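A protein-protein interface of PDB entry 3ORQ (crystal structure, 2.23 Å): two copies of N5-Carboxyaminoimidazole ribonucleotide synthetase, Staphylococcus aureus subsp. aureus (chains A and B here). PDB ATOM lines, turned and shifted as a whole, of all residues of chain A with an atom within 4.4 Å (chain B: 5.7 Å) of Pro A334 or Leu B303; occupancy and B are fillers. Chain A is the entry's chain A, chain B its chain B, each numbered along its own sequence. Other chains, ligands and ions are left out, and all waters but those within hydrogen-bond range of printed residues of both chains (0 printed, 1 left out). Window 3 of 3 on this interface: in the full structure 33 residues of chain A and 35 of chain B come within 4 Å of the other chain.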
ATOM      1  N   GLU A 332       3.867  33.578   3.876  1.00  0.00           N
ATOM      2  CA  GLU A 332       4.718  33.132   2.763  1.00  0.00           C
ATOM      3  C   GLU A 332       5.991  32.441   3.262  1.00  0.00           C
ATOM      4  O   GLU A 332       6.893  32.148   2.484  1.00  0.00           O
ATOM      5  CB  GLU A 332       5.038  34.288   1.774  1.00  0.00           C
ATOM      6  CG  GLU A 332       5.509  35.576   2.433  1.00  0.00           C
ATOM      7  CD  GLU A 332       5.734  36.771   1.449  1.00  0.00           C
ATOM      8  OE1 GLU A 332       4.847  37.655   1.350  1.00  0.00           O
ATOM      9  OE2 GLU A 332       6.812  36.840   0.813  1.00  0.00           O
ATOM     10  N   HIS A 333       6.045  32.183   4.566  1.00  0.00           N
ATOM     11  CA  HIS A 333       7.243  31.683   5.208  1.00  0.00           C
ATOM     12  C   HIS A 333       6.977  30.534   6.157  1.00  0.00           C
ATOM     13  O   HIS A 333       7.159  30.683   7.377  1.00  0.00           O
ATOM     14  CB  HIS A 333       7.881  32.807   5.953  1.00  0.00           C
ATOM     15  CG  HIS A 333       8.526  33.825   5.065  1.00  0.00           C
ATOM     16  ND1 HIS A 333       9.806  33.679   4.571  1.00  0.00           N
ATOM     17  CD2 HIS A 333       8.088  35.025   4.625  1.00  0.00           C
ATOM     18  CE1 HIS A 333      10.118  34.736   3.848  1.00  0.00           C
ATOM     19  NE2 HIS A 333       9.089  35.561   3.855  1.00  0.00           N
ATOM     20  N   PRO A 334       6.526  29.387   5.609  1.00  0.00           N
ATOM     21  CA  PRO A 334       6.269  28.208   6.394  1.00  0.00           C
ATOM     22  C   PRO A 334       7.536  27.732   7.134  1.00  0.00           C
ATOM     23  O   PRO A 334       7.413  27.090   8.177  1.00  0.00           O
ATOM     24  CB  PRO A 334       5.838  27.175   5.336  1.00  0.00           C
ATOM     25  CG  PRO A 334       6.504  27.663   4.038  1.00  0.00           C
ATOM     26  CD  PRO A 334       6.418  29.129   4.159  1.00  0.00           C
ATOM     27  N   GLU A 335       8.718  28.080   6.627  1.00  0.00           N
ATOM     28  CA  GLU A 335      10.001  27.699   7.242  1.00  0.00           C
ATOM     29  C   GLU A 335      10.271  28.490   8.523  1.00  0.00           C
ATOM     30  O   GLU A 335      11.287  28.260   9.170  1.00  0.00           O
ATOM     31  CB  GLU A 335      11.200  27.795   6.248  1.00  0.00           C
ATOM     32  CG  GLU A 335      11.586  29.217   5.839  1.00  0.00           C
ATOM     33  CD  GLU A 335      10.755  29.810   4.681  1.00  0.00           C
ATOM     34  OE1 GLU A 335       9.616  29.380   4.438  1.00  0.00           O
ATOM     35  OE2 GLU A 335      11.248  30.733   4.003  1.00  0.00           O
ATOM     36  N   TRP A 336       9.368  29.400   8.896  1.00  0.00           N
ATOM     37  CA  TRP A 336       9.498  30.086  10.168  1.00  0.00           C
ATOM     38  C   TRP A 336       8.893  29.324  11.373  1.00  0.00           C
ATOM     39  O   TRP A 336       9.166  29.676  12.526  1.00  0.00           O
ATOM     40  CB  TRP A 336       8.931  31.510  10.063  1.00  0.00           C
ATOM     41  CG  TRP A 336       9.805  32.433   9.202  1.00  0.00           C
ATOM     42  CD1 TRP A 336      10.999  32.113   8.586  1.00  0.00           C
ATOM     43  CD2 TRP A 336       9.571  33.813   8.916  1.00  0.00           C
ATOM     44  NE1 TRP A 336      11.483  33.192   7.927  1.00  0.00           N
ATOM     45  CE2 TRP A 336      10.642  34.255   8.105  1.00  0.00           C
ATOM     46  CE3 TRP A 336       8.548  34.714   9.252  1.00  0.00           C
ATOM     47  CZ2 TRP A 336      10.748  35.583   7.626  1.00  0.00           C
ATOM     48  CZ3 TRP A 336       8.641  36.055   8.770  1.00  0.00           C
ATOM     49  CH2 TRP A 336       9.742  36.467   7.958  1.00  0.00           C
ATOM     50  N   HIS A 337       8.110  28.282  11.121  1.00  0.00           N
ATOM     51  CA  HIS A 337       7.484  27.468  12.195  1.00  0.00           C
ATOM     52  C   HIS A 337       6.995  28.399  13.295  1.00  0.00           C
ATOM     53  O   HIS A 337       7.584  28.485  14.389  1.00  0.00           O
ATOM     54  CB  HIS A 337       8.432  26.408  12.775  1.00  0.00           C
ATOM     55  CG  HIS A 337       8.830  25.321  11.803  1.00  0.00           C
ATOM     56  ND1 HIS A 337      10.030  25.328  11.117  1.00  0.00           N
ATOM     57  CD2 HIS A 337       8.186  24.204  11.410  1.00  0.00           C
ATOM     58  CE1 HIS A 337      10.106  24.268  10.334  1.00  0.00           C
ATOM     59  NE2 HIS A 337       9.005  23.556  10.511  1.00  0.00           N
ATOM     60  N   THR B 200      -0.075  16.995   1.370  1.00  0.00           N
ATOM     61  CA  THR B 200      -0.859  18.190   1.636  1.00  0.00           C
ATOM     62  C   THR B 200      -0.987  19.075   0.404  1.00  0.00           C
ATOM     63  O   THR B 200       0.013  19.379  -0.269  1.00  0.00           O
ATOM     64  CB  THR B 200      -0.256  19.033   2.778  1.00  0.00           C
ATOM     65  OG1 THR B 200       0.005  18.205   3.935  1.00  0.00           O
ATOM     66  CG2 THR B 200      -1.241  20.121   3.194  1.00  0.00           C
ATOM     67  N   ARG B 201      -2.217  19.519   0.131  1.00  0.00           N
ATOM     68  CA  ARG B 201      -2.461  20.360  -1.021  1.00  0.00           C
ATOM     69  C   ARG B 201      -3.040  21.673  -0.556  1.00  0.00           C
ATOM     70  O   ARG B 201      -3.904  21.678   0.285  1.00  0.00           O
ATOM     71  CB  ARG B 201      -3.359  19.654  -2.043  1.00  0.00           C
ATOM     72  CG  ARG B 201      -3.762  20.542  -3.198  1.00  0.00           C
ATOM     73  CD  ARG B 201      -4.206  19.751  -4.418  1.00  0.00           C
ATOM     74  NE  ARG B 201      -4.381  20.678  -5.530  1.00  0.00           N
ATOM     75  CZ  ARG B 201      -5.420  21.500  -5.663  1.00  0.00           C
ATOM     76  NH1 ARG B 201      -6.456  21.502  -4.795  1.00  0.00           N
ATOM     77  NH2 ARG B 201      -5.434  22.322  -6.686  1.00  0.00           N
ATOM     78  N   GLY B 202      -2.514  22.785  -1.041  1.00  0.00           N
ATOM     79  CA  GLY B 202      -2.923  24.094  -0.504  1.00  0.00           C
ATOM     80  C   GLY B 202      -3.471  25.036  -1.572  1.00  0.00           C
ATOM     81  O   GLY B 202      -3.699  24.631  -2.705  1.00  0.00           O
ATOM     82  N   GLN B 206      -0.243  24.383  -4.712  1.00  0.00           N
ATOM     83  CA  GLN B 206       0.894  23.891  -3.958  1.00  0.00           C
ATOM     84  C   GLN B 206       0.610  22.473  -3.438  1.00  0.00           C
ATOM     85  O   GLN B 206      -0.450  22.224  -2.864  1.00  0.00           O
ATOM     86  CB  GLN B 206       1.122  24.796  -2.779  1.00  0.00           C
ATOM     87  CG  GLN B 206       2.075  25.926  -2.963  1.00  0.00           C
ATOM     88  CD  GLN B 206       2.435  26.481  -1.599  1.00  0.00           C
ATOM     89  OE1 GLN B 206       1.565  27.020  -0.891  1.00  0.00           O
ATOM     90  NE2 GLN B 206       3.702  26.294  -1.193  1.00  0.00           N
ATOM     91  N   ILE B 207       1.570  21.574  -3.638  1.00  0.00           N
ATOM     92  CA  ILE B 207       1.480  20.164  -3.276  1.00  0.00           C
ATOM     93  C   ILE B 207       2.805  19.761  -2.614  1.00  0.00           C
ATOM     94  O   ILE B 207       3.897  19.987  -3.163  1.00  0.00           O
ATOM     95  CB  ILE B 207       1.233  19.293  -4.515  1.00  0.00           C
ATOM     96  CG1 ILE B 207      -0.210  19.452  -5.017  1.00  0.00           C
ATOM     97  CG2 ILE B 207       1.460  17.830  -4.221  1.00  0.00           C
ATOM     98  CD1 ILE B 207      -0.452  18.776  -6.384  1.00  0.00           C
ATOM     99  N   THR B 208       2.720  19.188  -1.422  1.00  0.00           N
ATOM    100  CA  THR B 208       3.924  18.815  -0.697  1.00  0.00           C
ATOM    101  C   THR B 208       3.798  17.348  -0.247  1.00  0.00           C
ATOM    102  O   THR B 208       2.733  16.934   0.268  1.00  0.00           O
ATOM    103  CB  THR B 208       4.196  19.784   0.491  1.00  0.00           C
ATOM    104  OG1 THR B 208       5.446  19.465   1.087  1.00  0.00           O
ATOM    105  CG2 THR B 208       3.179  19.623   1.569  1.00  0.00           C
ATOM    106  N   TYR B 288       7.962  19.055   9.726  1.00  0.00           N
ATOM    107  CA  TYR B 288       6.548  19.483   9.797  1.00  0.00           C
ATOM    108  C   TYR B 288       5.751  18.220  10.031  1.00  0.00           C
ATOM    109  O   TYR B 288       6.130  17.173   9.521  1.00  0.00           O
ATOM    110  CB  TYR B 288       6.048  20.065   8.440  1.00  0.00           C
ATOM    111  CG  TYR B 288       6.782  21.309   8.015  1.00  0.00           C
ATOM    112  CD1 TYR B 288       8.018  21.211   7.301  1.00  0.00           C
ATOM    113  CD2 TYR B 288       6.268  22.584   8.306  1.00  0.00           C
ATOM    114  CE1 TYR B 288       8.724  22.345   6.931  1.00  0.00           C
ATOM    115  CE2 TYR B 288       6.975  23.759   7.912  1.00  0.00           C
ATOM    116  CZ  TYR B 288       8.205  23.623   7.235  1.00  0.00           C
ATOM    117  OH  TYR B 288       8.914  24.750   6.816  1.00  0.00           O
ATOM    118  N   THR B 293       0.902  20.907   8.518  1.00  0.00           N
ATOM    119  CA  THR B 293       0.666  21.307   7.135  1.00  0.00           C
ATOM    120  C   THR B 293      -0.847  21.355   6.824  1.00  0.00           C
ATOM    121  O   THR B 293      -1.276  22.121   5.982  1.00  0.00           O
ATOM    122  CB  THR B 293       1.377  20.393   6.131  1.00  0.00           C
ATOM    123  OG1 THR B 293       0.926  19.047   6.295  1.00  0.00           O
ATOM    124  CG2 THR B 293       2.889  20.472   6.288  1.00  0.00           C
ATOM    125  N   LEU B 296      -1.943  24.929   7.978  1.00  0.00           N
ATOM    126  CA  LEU B 296      -1.440  25.834   6.963  1.00  0.00           C
ATOM    127  C   LEU B 296      -2.281  25.836   5.703  1.00  0.00           C
ATOM    128  O   LEU B 296      -2.648  26.882   5.212  1.00  0.00           O
ATOM    129  CB  LEU B 296       0.012  25.469   6.582  1.00  0.00           C
ATOM    130  CG  LEU B 296       1.142  25.688   7.599  1.00  0.00           C
ATOM    131  CD1 LEU B 296       2.476  25.155   7.019  1.00  0.00           C
ATOM    132  CD2 LEU B 296       1.252  27.146   7.998  1.00  0.00           C
ATOM    133  N   ALA B 297      -2.510  24.665   5.132  1.00  0.00           N
ATOM    134  CA  ALA B 297      -3.212  24.541   3.857  1.00  0.00           C
ATOM    135  C   ALA B 297      -4.591  25.144   4.005  1.00  0.00           C
ATOM    136  O   ALA B 297      -5.019  26.025   3.236  1.00  0.00           O
ATOM    137  CB  ALA B 297      -3.372  23.118   3.522  1.00  0.00           C
ATOM    138  N   GLN B 301      -2.332  29.485   3.974  1.00  0.00           N
ATOM    139  CA  GLN B 301      -0.926  29.854   4.075  1.00  0.00           C
ATOM    140  C   GLN B 301      -0.107  29.103   3.031  1.00  0.00           C
ATOM    141  O   GLN B 301      -0.567  28.102   2.483  1.00  0.00           O
ATOM    142  CB  GLN B 301      -0.390  29.531   5.452  1.00  0.00           C
ATOM    143  CG  GLN B 301      -1.344  29.847   6.588  1.00  0.00           C
ATOM    144  CD  GLN B 301      -1.558  31.329   6.708  1.00  0.00           C
ATOM    145  OE1 GLN B 301      -0.608  32.101   6.700  1.00  0.00           O
ATOM    146  NE2 GLN B 301      -2.800  31.736   6.798  1.00  0.00           N
ATOM    147  N   SER B 302       1.103  29.568   2.749  1.00  0.00           N
ATOM    148  CA  SER B 302       2.007  28.796   1.893  1.00  0.00           C
ATOM    149  C   SER B 302       2.461  27.516   2.610  1.00  0.00           C
ATOM    150  O   SER B 302       2.715  27.544   3.806  1.00  0.00           O
ATOM    151  CB  SER B 302       3.270  29.588   1.534  1.00  0.00           C
ATOM    152  OG  SER B 302       3.005  30.537   0.563  1.00  0.00           O
ATOM    153  N   LEU B 303       2.605  26.439   1.853  1.00  0.00           N
ATOM    154  CA  LEU B 303       3.148  25.162   2.338  1.00  0.00           C
ATOM    155  C   LEU B 303       4.675  25.061   2.130  1.00  0.00           C
ATOM    156  O   LEU B 303       5.205  25.632   1.196  1.00  0.00           O
ATOM    157  CB  LEU B 303       2.492  24.025   1.557  1.00  0.00           C
ATOM    158  CG  LEU B 303       0.987  23.968   1.766  1.00  0.00           C
ATOM    159  CD1 LEU B 303       0.413  22.827   0.989  1.00  0.00           C
ATOM    160  CD2 LEU B 303       0.642  23.837   3.302  1.00  0.00           C
ATOM    161  N   PRO B 304       5.381  24.294   2.974  1.00  0.00           N
ATOM    162  CA  PRO B 304       6.782  24.107   2.609  1.00  0.00           C
ATOM    163  C   PRO B 304       6.900  23.317   1.298  1.00  0.00           C
ATOM    164  O   PRO B 304       5.987  22.564   0.950  1.00  0.00           O
ATOM    165  CB  PRO B 304       7.358  23.310   3.799  1.00  0.00           C
ATOM    166  CG  PRO B 304       6.155  22.546   4.324  1.00  0.00           C
ATOM    167  CD  PRO B 304       4.979  23.485   4.134  1.00  0.00           C
ATOM    168  N   ASN B 305       8.006  23.500   0.576  1.00  0.00           N
ATOM    169  CA  ASN B 305       8.208  22.838  -0.722  1.00  0.00           C
ATOM    170  C   ASN B 305       8.568  21.367  -0.586  1.00  0.00           C
ATOM    171  O   ASN B 305       8.352  20.586  -1.506  1.00  0.00           O
ATOM    172  CB  ASN B 305       9.302  23.538  -1.548  1.00  0.00           C
ATOM    173  CG  ASN B 305       8.876  24.933  -2.021  1.00  0.00           C
ATOM    174  OD1 ASN B 305       7.711  25.162  -2.381  1.00  0.00           O
ATOM    175  ND2 ASN B 305       9.823  25.872  -2.006  1.00  0.00           N
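Among the printed residues, pairs that only touch across the chains: Glu A332 with Ser B302 (3.8 Å), Pro A334 with Ser B302 (3.5 Å), Pro A334 with Leu B303 (3.7 Å), Pro A334 with Pro B304 (3.7 Å) and His A337 with Tyr B288 (3.3 Å).
N of Glu A335 sits close to OH of Tyr B288 (3.3 Å).
O of Pro A334 lies within hydrogen-bond range of OH of Tyr B288 (3.1 Å).
No position is printed for both chains.
Of the 7 pairs that touch across the chains among the printed residues, none has its exchanged pair printed and touching as well.
The backbone carbonyl oxygen (O) of Pro B304 sits at hydrogen-bond distance from the side-chain hydroxyl (OG1) of Thr B208 (3.1 Å).
The backbone carbonyl oxygen of Leu B303 lies within hydrogen-bond range of the side-chain amide nitrogen of Gln B206, at 2.9 Å.
ND1 of His A333 is in hydrogen-bond range of OE2 of Glu A335 (3.3 Å).
Printed residues of chain B that touch a printed residue of chain A: Tyr B288, Ser B302, Leu B303 and Pro B304.
Of the 6 printed residues of chain A, 4 touch a printed residue of chain B.
Among the printed residues, 7 pairs touch across the chains.
Among the printed residues, no Asp or Glu carboxylate lies within 4 Å of a Lys or Arg side-chain nitrogen of the other chain.
Printed residues of chain B within 4 Å of Glu A332: Ser B302.
Pro A334 touches four residues of chain B.
Of the printed residues of chain B, His A337 touches Tyr B288.
Printed residues of chain A within 4 Å of Tyr B288: Pro A334 (3.1 Å), Glu A335 (3.2 Å) and His A337 (3.3 Å).
Of the printed residues of chain A, Ser B302 touches Glu A332 and Pro A334.
Of chain A, only Pro A334 (3.7 Å) comes within 4 Å of Leu B303.
The nearest residue of chain B that does not touch Pro A334 is Leu B296 (4.3 Å).
The nearest printed residue of chain A that does not touch Leu B303 is Glu A335 (6.6 Å).
The nearest printed residue of chain B that does not touch His A337 is Pro B304 (6.9 Å).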
